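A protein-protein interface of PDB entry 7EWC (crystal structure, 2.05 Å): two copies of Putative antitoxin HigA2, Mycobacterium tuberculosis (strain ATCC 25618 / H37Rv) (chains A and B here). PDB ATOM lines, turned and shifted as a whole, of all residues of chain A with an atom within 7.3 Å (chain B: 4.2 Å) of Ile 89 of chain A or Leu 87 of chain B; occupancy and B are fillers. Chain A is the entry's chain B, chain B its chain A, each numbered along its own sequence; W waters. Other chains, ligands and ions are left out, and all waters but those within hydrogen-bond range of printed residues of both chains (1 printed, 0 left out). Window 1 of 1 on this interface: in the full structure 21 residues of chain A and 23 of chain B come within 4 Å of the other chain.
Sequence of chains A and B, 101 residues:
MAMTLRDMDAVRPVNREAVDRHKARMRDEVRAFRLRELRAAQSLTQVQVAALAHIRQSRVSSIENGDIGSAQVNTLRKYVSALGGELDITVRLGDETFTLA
The side-chain carboxylate (OE2) of Glu 86 of chain B lies within salt-bridge range of the guanidinium group (NH2) of Arg 92 of chain A (3.3 Å). N of Asp 88 of chain B sits at hydrogen-bond distance from O of Thr 90 of chain A. NH1 of Arg 92 of chain A is in salt-bridge range of OD2 of Asp 88 of chain B, 2.6 Å away.
The backbone carbonyl oxygen (O) of Leu 87 of chain B is in hydrogen-bond range of the guanidinium group (NH1) of Arg 77 of chain B (3.5 Å). The guanidinium group of Arg 77 of chain A sits at hydrogen-bond distance from the backbone carbonyl oxygen of Leu 87 of chain A (3.2 Å). The backbone carbonyl oxygen (O) of Ile 89 of chain A is in hydrogen-bond range of the backbone NH (N) of Leu 100 of chain A (2.7 Å). The backbone carbonyl oxygen (O) of Ala 101 of chain A sits at hydrogen-bond distance from the backbone NH (N) of Ile 89 of chain A (2.9 Å). N of Val 91 of chain A lies within hydrogen-bond range of O of Phe 98 of chain A (2.8 Å).
Among the printed residues, merely in contact across the chains: Leu 87 of chain A with Ile 89 of chain B, Asp 88 of chain A with Asp 88 of chain B, Asp 88 of chain A with Ile 89 of chain B, Ile 89 of chain A with Leu 87 of chain B, Ile 89 of chain A with Asp 88 of chain B, Thr 90 of chain A with Glu 86 of chain B, Thr 90 of chain A with Leu 87 of chain B, Val 91 of chain A with Val 80 of chain B, Val 91 of chain A with Glu 86 of chain B and Leu 100 of chain A with Leu 76 of chain B.
Arg 77 of chain A touches none of the printed residues of chain B. Printed residues of chain B within 4 Å of Asp 88 of chain A: Asp 88 (3.5 Å) and Ile 89 (3.4 Å). Of chain B, only Leu 87 (3.5 Å) and Asp 88 (3.5 Å) come within 4 Å of Ile 89 of chain A. Printed residues of chain A within 4 Å of Leu 76 of chain B: Leu 100. Of the printed residues of chain A, Val 80 of chain B touches Val 91. Printed residues of chain A within 4 Å of Glu 86 of chain B: Thr 90, Val 91 and Arg 92. Of chain A, only Ile 89 and Thr 90 come within 4 Å of Leu 87 of chain B. The nearest printed residue of chain B that does not touch Ile 89 of chain A is Ile 89 of chain B (4.2 Å). The nearest printed residue of chain A that does not touch Leu 87 of chain B is Leu 100 of chain A (4.2 Å).
Printed residues of chain B that touch a printed residue of chain A: Leu 76, Val 80, Glu 86, Leu 87, Asp 88 and Ile 89. Hydrophobic or aromatic side chains of chain B that line the printed part of chain A: Leu 76, Val 80, Leu 87 and Ile 89. Of the 14 printed residues of chain A, 7 touch a printed residue of chain B. Hydrophobic or aromatic side chains of chain A that line the printed part of chain B: Leu 87, Ile 89, Val 91 and Leu 100. Among the printed residues, 13 pairs touch across the chains.
Leu 87 of chain A touches Ile 89 of chain B, and with the chains exchanged Ile 89 of chain A touches Leu 87 of chain B. Asp 88 of chain B touches its own counterpart, Asp 88 of chain A. Asp 88 of chain A touches Ile 89 of chain B, and with the chains exchanged Ile 89 of chain A touches Asp 88 of chain B.
Water W1 bridges the backbone carbonyl oxygen (O) of Asp 88 of chain B (2.7 Å) and the backbone carbonyl oxygen (O) of Asp 88 of chain A (3.0 Å).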
ATOM      1  N   VAL A  73     -21.006  23.666 -20.707  1.00  0.00           N
ATOM      2  CA  VAL A  73     -21.921  22.651 -21.304  1.00  0.00           C
ATOM      3  C   VAL A  73     -22.549  23.194 -22.600  1.00  0.00           C
ATOM      4  O   VAL A  73     -22.663  22.399 -23.539  1.00  0.00           O
ATOM      5  CB  VAL A  73     -22.980  22.224 -20.275  1.00  0.00           C
ATOM      6  CG1 VAL A  73     -24.203  21.563 -20.895  1.00  0.00           C
ATOM      7  CG2 VAL A  73     -22.345  21.328 -19.221  1.00  0.00           C
ATOM      8  N   ASN A  74     -22.987  24.461 -22.653  1.00  0.00           N
ATOM      9  CA  ASN A  74     -23.711  24.985 -23.851  1.00  0.00           C
ATOM     10  C   ASN A  74     -22.697  25.098 -25.002  1.00  0.00           C
ATOM     11  O   ASN A  74     -23.029  24.661 -26.109  1.00  0.00           O
ATOM     12  CB  ASN A  74     -24.554  26.240 -23.564  1.00  0.00           C
ATOM     13  CG  ASN A  74     -26.014  25.918 -23.283  1.00  0.00           C
ATOM     14  OD1 ASN A  74     -26.424  24.752 -23.315  1.00  0.00           O
ATOM     15  ND2 ASN A  74     -26.812  26.936 -22.995  1.00  0.00           N
ATOM     16  N   LEU A  76     -19.919  23.151 -25.432  1.00  0.00           N
ATOM     17  CA  LEU A  76     -19.660  21.751 -25.874  1.00  0.00           C
ATOM     18  C   LEU A  76     -20.867  21.225 -26.664  1.00  0.00           C
ATOM     19  O   LEU A  76     -20.670  20.497 -27.672  1.00  0.00           O
ATOM     20  CB  LEU A  76     -19.367  20.908 -24.625  1.00  0.00           C
ATOM     21  CG  LEU A  76     -18.998  19.453 -24.862  1.00  0.00           C
ATOM     22  CD1 LEU A  76     -17.727  19.315 -25.700  1.00  0.00           C
ATOM     23  CD2 LEU A  76     -18.817  18.731 -23.523  1.00  0.00           C
ATOM     24  N   ARG A  77     -22.077  21.546 -26.216  1.00  0.00           N
ATOM     25  CA  ARG A  77     -23.347  21.157 -26.891  1.00  0.00           C
ATOM     26  C   ARG A  77     -23.353  21.699 -28.337  1.00  0.00           C
ATOM     27  O   ARG A  77     -23.651  20.945 -29.286  1.00  0.00           O
ATOM     28  CB  ARG A  77     -24.514  21.689 -26.045  1.00  0.00           C
ATOM     29  CG  ARG A  77     -25.908  21.546 -26.643  1.00  0.00           C
ATOM     30  CD  ARG A  77     -26.994  21.595 -25.563  1.00  0.00           C
ATOM     31  NE  ARG A  77     -26.806  20.479 -24.635  1.00  0.00           N
ATOM     32  CZ  ARG A  77     -27.052  19.189 -24.913  1.00  0.00           C
ATOM     33  NH1 ARG A  77     -27.547  18.825 -26.085  1.00  0.00           N
ATOM     34  NH2 ARG A  77     -26.801  18.249 -24.017  1.00  0.00           N
ATOM     35  N   LEU A  87     -24.986  15.610 -27.928  1.00  0.00           N
ATOM     36  CA  LEU A  87     -24.333  15.502 -26.601  1.00  0.00           C
ATOM     37  C   LEU A  87     -25.362  14.971 -25.592  1.00  0.00           C
ATOM     38  O   LEU A  87     -26.461  15.481 -25.552  1.00  0.00           O
ATOM     39  CB  LEU A  87     -23.791  16.865 -26.178  1.00  0.00           C
ATOM     40  CG  LEU A  87     -23.002  16.865 -24.868  1.00  0.00           C
ATOM     41  CD1 LEU A  87     -21.620  16.273 -25.054  1.00  0.00           C
ATOM     42  CD2 LEU A  87     -22.911  18.261 -24.318  1.00  0.00           C
ATOM     43  N   ASP A  88     -24.990  13.952 -24.832  1.00  0.00           N
ATOM     44  CA  ASP A  88     -25.782  13.433 -23.689  1.00  0.00           C
ATOM     45  C   ASP A  88     -25.020  13.707 -22.403  1.00  0.00           C
ATOM     46  O   ASP A  88     -23.852  13.358 -22.311  1.00  0.00           O
ATOM     47  CB  ASP A  88     -26.060  11.953 -23.867  1.00  0.00           C
ATOM     48  CG  ASP A  88     -27.025  11.725 -25.011  1.00  0.00           C
ATOM     49  OD1 ASP A  88     -27.890  12.595 -25.232  1.00  0.00           O
ATOM     50  OD2 ASP A  88     -26.874  10.704 -25.700  1.00  0.00           O
ATOM     51  N   ILE A  89     -25.666  14.348 -21.446  1.00  0.00           N
ATOM     52  CA  ILE A  89     -25.132  14.443 -20.072  1.00  0.00           C
ATOM     53  C   ILE A  89     -26.077  13.675 -19.160  1.00  0.00           C
ATOM     54  O   ILE A  89     -27.260  14.036 -19.137  1.00  0.00           O
ATOM     55  CB  ILE A  89     -24.960  15.903 -19.666  1.00  0.00           C
ATOM     56  CG1 ILE A  89     -24.225  16.666 -20.771  1.00  0.00           C
ATOM     57  CG2 ILE A  89     -24.245  15.977 -18.331  1.00  0.00           C
ATOM     58  CD1 ILE A  89     -23.896  18.094 -20.411  1.00  0.00           C
ATOM     59  N   THR A  90     -25.581  12.622 -18.496  1.00  0.00           N
ATOM     60  CA  THR A  90     -26.435  11.816 -17.588  1.00  0.00           C
ATOM     61  C   THR A  90     -25.780  11.694 -16.212  1.00  0.00           C
ATOM     62  O   THR A  90     -24.554  11.509 -16.133  1.00  0.00           O
ATOM     63  CB  THR A  90     -26.839  10.466 -18.195  1.00  0.00           C
ATOM     64  OG1 THR A  90     -25.827   9.521 -17.898  1.00  0.00           O
ATOM     65  CG2 THR A  90     -27.071  10.516 -19.684  1.00  0.00           C
ATOM     66  N   VAL A  91     -26.615  11.798 -15.176  1.00  0.00           N
ATOM     67  CA  VAL A  91     -26.226  11.530 -13.770  1.00  0.00           C
ATOM     68  C   VAL A  91     -26.563  10.079 -13.485  1.00  0.00           C
ATOM     69  O   VAL A  91     -27.692   9.646 -13.780  1.00  0.00           O
ATOM     70  CB  VAL A  91     -26.934  12.484 -12.807  1.00  0.00           C
ATOM     71  CG1 VAL A  91     -26.542  12.206 -11.359  1.00  0.00           C
ATOM     72  CG2 VAL A  91     -26.643  13.918 -13.211  1.00  0.00           C
ATOM     73  N   ARG A  92     -25.584   9.359 -12.974  1.00  0.00           N
ATOM     74  CA  ARG A  92     -25.775   7.979 -12.520  1.00  0.00           C
ATOM     75  C   ARG A  92     -25.575   7.944 -11.013  1.00  0.00           C
ATOM     76  O   ARG A  92     -24.515   8.414 -10.541  1.00  0.00           O
ATOM     77  CB  ARG A  92     -24.774   7.105 -13.259  1.00  0.00           C
ATOM     78  CG  ARG A  92     -24.446   5.821 -12.542  1.00  0.00           C
ATOM     79  CD  ARG A  92     -23.846   4.812 -13.508  1.00  0.00           C
ATOM     80  NE  ARG A  92     -22.406   5.005 -13.615  1.00  0.00           N
ATOM     81  CZ  ARG A  92     -21.826   5.706 -14.574  1.00  0.00           C
ATOM     82  NH1 ARG A  92     -22.574   6.243 -15.518  1.00  0.00           N
ATOM     83  NH2 ARG A  92     -20.512   5.860 -14.604  1.00  0.00           N
ATOM     84  N   PHE A  98     -30.410   9.774 -14.868  1.00  0.00           N
ATOM     85  CA  PHE A  98     -31.272  10.769 -15.550  1.00  0.00           C
ATOM     86  C   PHE A  98     -30.417  11.804 -16.270  1.00  0.00           C
ATOM     87  O   PHE A  98     -29.292  12.097 -15.804  1.00  0.00           O
ATOM     88  CB  PHE A  98     -32.214  11.475 -14.581  1.00  0.00           C
ATOM     89  CG  PHE A  98     -31.526  12.249 -13.490  1.00  0.00           C
ATOM     90  CD1 PHE A  98     -31.260  13.603 -13.646  1.00  0.00           C
ATOM     91  CD2 PHE A  98     -31.182  11.625 -12.301  1.00  0.00           C
ATOM     92  CE1 PHE A  98     -30.631  14.321 -12.641  1.00  0.00           C
ATOM     93  CE2 PHE A  98     -30.584  12.353 -11.286  1.00  0.00           C
ATOM     94  CZ  PHE A  98     -30.295  13.695 -11.460  1.00  0.00           C
ATOM     95  N   THR A  99     -30.980  12.327 -17.362  1.00  0.00           N
ATOM     96  CA  THR A  99     -30.343  13.271 -18.308  1.00  0.00           C
ATOM     97  C   THR A  99     -30.310  14.643 -17.669  1.00  0.00           C
ATOM     98  O   THR A  99     -31.288  14.982 -17.006  1.00  0.00           O
ATOM     99  CB  THR A  99     -31.150  13.424 -19.608  1.00  0.00           C
ATOM    100  OG1 THR A  99     -31.838  12.203 -19.836  1.00  0.00           O
ATOM    101  CG2 THR A  99     -30.292  13.759 -20.804  1.00  0.00           C
ATOM    102  N   LEU A 100     -29.247  15.403 -17.907  1.00  0.00           N
ATOM    103  CA  LEU A 100     -29.165  16.839 -17.553  1.00  0.00           C
ATOM    104  C   LEU A 100     -29.259  17.712 -18.809  1.00  0.00           C
ATOM    105  O   LEU A 100     -29.731  18.869 -18.697  1.00  0.00           O
ATOM    106  CB  LEU A 100     -27.833  17.078 -16.846  1.00  0.00           C
ATOM    107  CG  LEU A 100     -27.817  16.729 -15.372  1.00  0.00           C
ATOM    108  CD1 LEU A 100     -26.568  17.283 -14.709  1.00  0.00           C
ATOM    109  CD2 LEU A 100     -29.064  17.252 -14.688  1.00  0.00           C
ATOM    110  N   ALA A 101     -28.760  17.201 -19.934  1.00  0.00           N
ATOM    111  CA  ALA A 101     -28.794  17.860 -21.258  1.00  0.00           C
ATOM    112  C   ALA A 101     -28.510  16.810 -22.338  1.00  0.00           C
ATOM    113  O   ALA A 101     -28.182  15.660 -21.996  1.00  0.00           O
ATOM    114  CB  ALA A 101     -27.813  19.016 -21.276  1.00  0.00           C
ATOM    115  N   LEU B  76     -19.672  20.844 -13.018  1.00  0.00           N
ATOM    116  CA  LEU B  76     -20.833  19.926 -12.966  1.00  0.00           C
ATOM    117  C   LEU B  76     -20.351  18.562 -12.437  1.00  0.00           C
ATOM    118  O   LEU B  76     -21.005  18.011 -11.541  1.00  0.00           O
ATOM    119  CB  LEU B  76     -21.478  19.863 -14.344  1.00  0.00           C
ATOM    120  CG  LEU B  76     -22.828  19.164 -14.409  1.00  0.00           C
ATOM    121  CD1 LEU B  76     -23.811  19.754 -13.394  1.00  0.00           C
ATOM    122  CD2 LEU B  76     -23.421  19.230 -15.812  1.00  0.00           C
ATOM    123  N   ARG B  77     -19.181  18.099 -12.860  1.00  0.00           N
ATOM    124  CA  ARG B  77     -18.653  16.782 -12.442  1.00  0.00           C
ATOM    125  C   ARG B  77     -18.501  16.782 -10.924  1.00  0.00           C
ATOM    126  O   ARG B  77     -19.005  15.838 -10.257  1.00  0.00           O
ATOM    127  CB  ARG B  77     -17.340  16.426 -13.143  1.00  0.00           C
ATOM    128  CG  ARG B  77     -16.692  15.183 -12.541  1.00  0.00           C
ATOM    129  CD  ARG B  77     -15.736  14.391 -13.427  1.00  0.00           C
ATOM    130  NE  ARG B  77     -15.610  15.015 -14.739  1.00  0.00           N
ATOM    131  CZ  ARG B  77     -16.222  14.611 -15.849  1.00  0.00           C
ATOM    132  NH1 ARG B  77     -16.990  13.524 -15.868  1.00  0.00           N
ATOM    133  NH2 ARG B  77     -16.021  15.302 -16.955  1.00  0.00           N
ATOM    134  N   VAL B  80     -21.917  16.862  -8.959  1.00  0.00           N
ATOM    135  CA  VAL B  80     -22.535  15.503  -9.001  1.00  0.00           C
ATOM    136  C   VAL B  80     -21.793  14.509  -8.095  1.00  0.00           C
ATOM    137  O   VAL B  80     -22.515  13.715  -7.391  1.00  0.00           O
ATOM    138  CB  VAL B  80     -22.678  15.056 -10.464  1.00  0.00           C
ATOM    139  CG1 VAL B  80     -23.126  13.591 -10.601  1.00  0.00           C
ATOM    140  CG2 VAL B  80     -23.673  15.982 -11.142  1.00  0.00           C
ATOM    141  N   GLU B  86     -22.168   9.937 -10.418  1.00  0.00           N
ATOM    142  CA  GLU B  86     -21.151   9.994 -11.481  1.00  0.00           C
ATOM    143  C   GLU B  86     -21.779  10.664 -12.687  1.00  0.00           C
ATOM    144  O   GLU B  86     -22.977  10.406 -13.006  1.00  0.00           O
ATOM    145  CB  GLU B  86     -20.603   8.605 -11.780  1.00  0.00           C
ATOM    146  CG  GLU B  86     -19.733   8.113 -10.640  1.00  0.00           C
ATOM    147  CD  GLU B  86     -18.457   7.435 -11.093  1.00  0.00           C
ATOM    148  OE1 GLU B  86     -17.404   7.716 -10.501  1.00  0.00           O
ATOM    149  OE2 GLU B  86     -18.529   6.620 -12.042  1.00  0.00           O
ATOM    150  N   LEU B  87     -21.033  11.575 -13.281  1.00  0.00           N
ATOM    151  CA  LEU B  87     -21.509  12.315 -14.479  1.00  0.00           C
ATOM    152  C   LEU B  87     -20.967  11.588 -15.706  1.00  0.00           C
ATOM    153  O   LEU B  87     -19.751  11.378 -15.766  1.00  0.00           O
ATOM    154  CB  LEU B  87     -21.010  13.756 -14.384  1.00  0.00           C
ATOM    155  CG  LEU B  87     -21.582  14.728 -15.412  1.00  0.00           C
ATOM    156  CD1 LEU B  87     -23.057  15.005 -15.183  1.00  0.00           C
ATOM    157  CD2 LEU B  87     -20.773  16.006 -15.414  1.00  0.00           C
ATOM    158  N   ASP B  88     -21.845  11.163 -16.611  1.00  0.00           N
ATOM    159  CA  ASP B  88     -21.451  10.557 -17.910  1.00  0.00           C
ATOM    160  C   ASP B  88     -21.736  11.575 -19.009  1.00  0.00           C
ATOM    161  O   ASP B  88     -22.922  11.929 -19.218  1.00  0.00           O
ATOM    162  CB  ASP B  88     -22.250   9.305 -18.279  1.00  0.00           C
ATOM    163  CG  ASP B  88     -21.658   8.024 -17.733  1.00  0.00           C
ATOM    164  OD1 ASP B  88     -20.604   8.093 -17.066  1.00  0.00           O
ATOM    165  OD2 ASP B  88     -22.275   6.960 -17.957  1.00  0.00           O
ATOM    166  N   ILE B  89     -20.693  11.981 -19.716  1.00  0.00           N
ATOM    167  CA  ILE B  89     -20.824  12.868 -20.907  1.00  0.00           C
ATOM    168  C   ILE B  89     -20.453  12.048 -22.143  1.00  0.00           C
ATOM    169  O   ILE B  89     -19.325  11.562 -22.233  1.00  0.00           O
ATOM    170  CB  ILE B  89     -19.969  14.126 -20.729  1.00  0.00           C
ATOM    171  CG1 ILE B  89     -20.393  14.875 -19.462  1.00  0.00           C
ATOM    172  CG2 ILE B  89     -20.067  15.008 -21.968  1.00  0.00           C
ATOM    173  CD1 ILE B  89     -19.423  15.939 -19.043  1.00  0.00           C
HETATM  174  O   HOH W   1     -24.221  10.641 -21.146  1.00  0.00           O
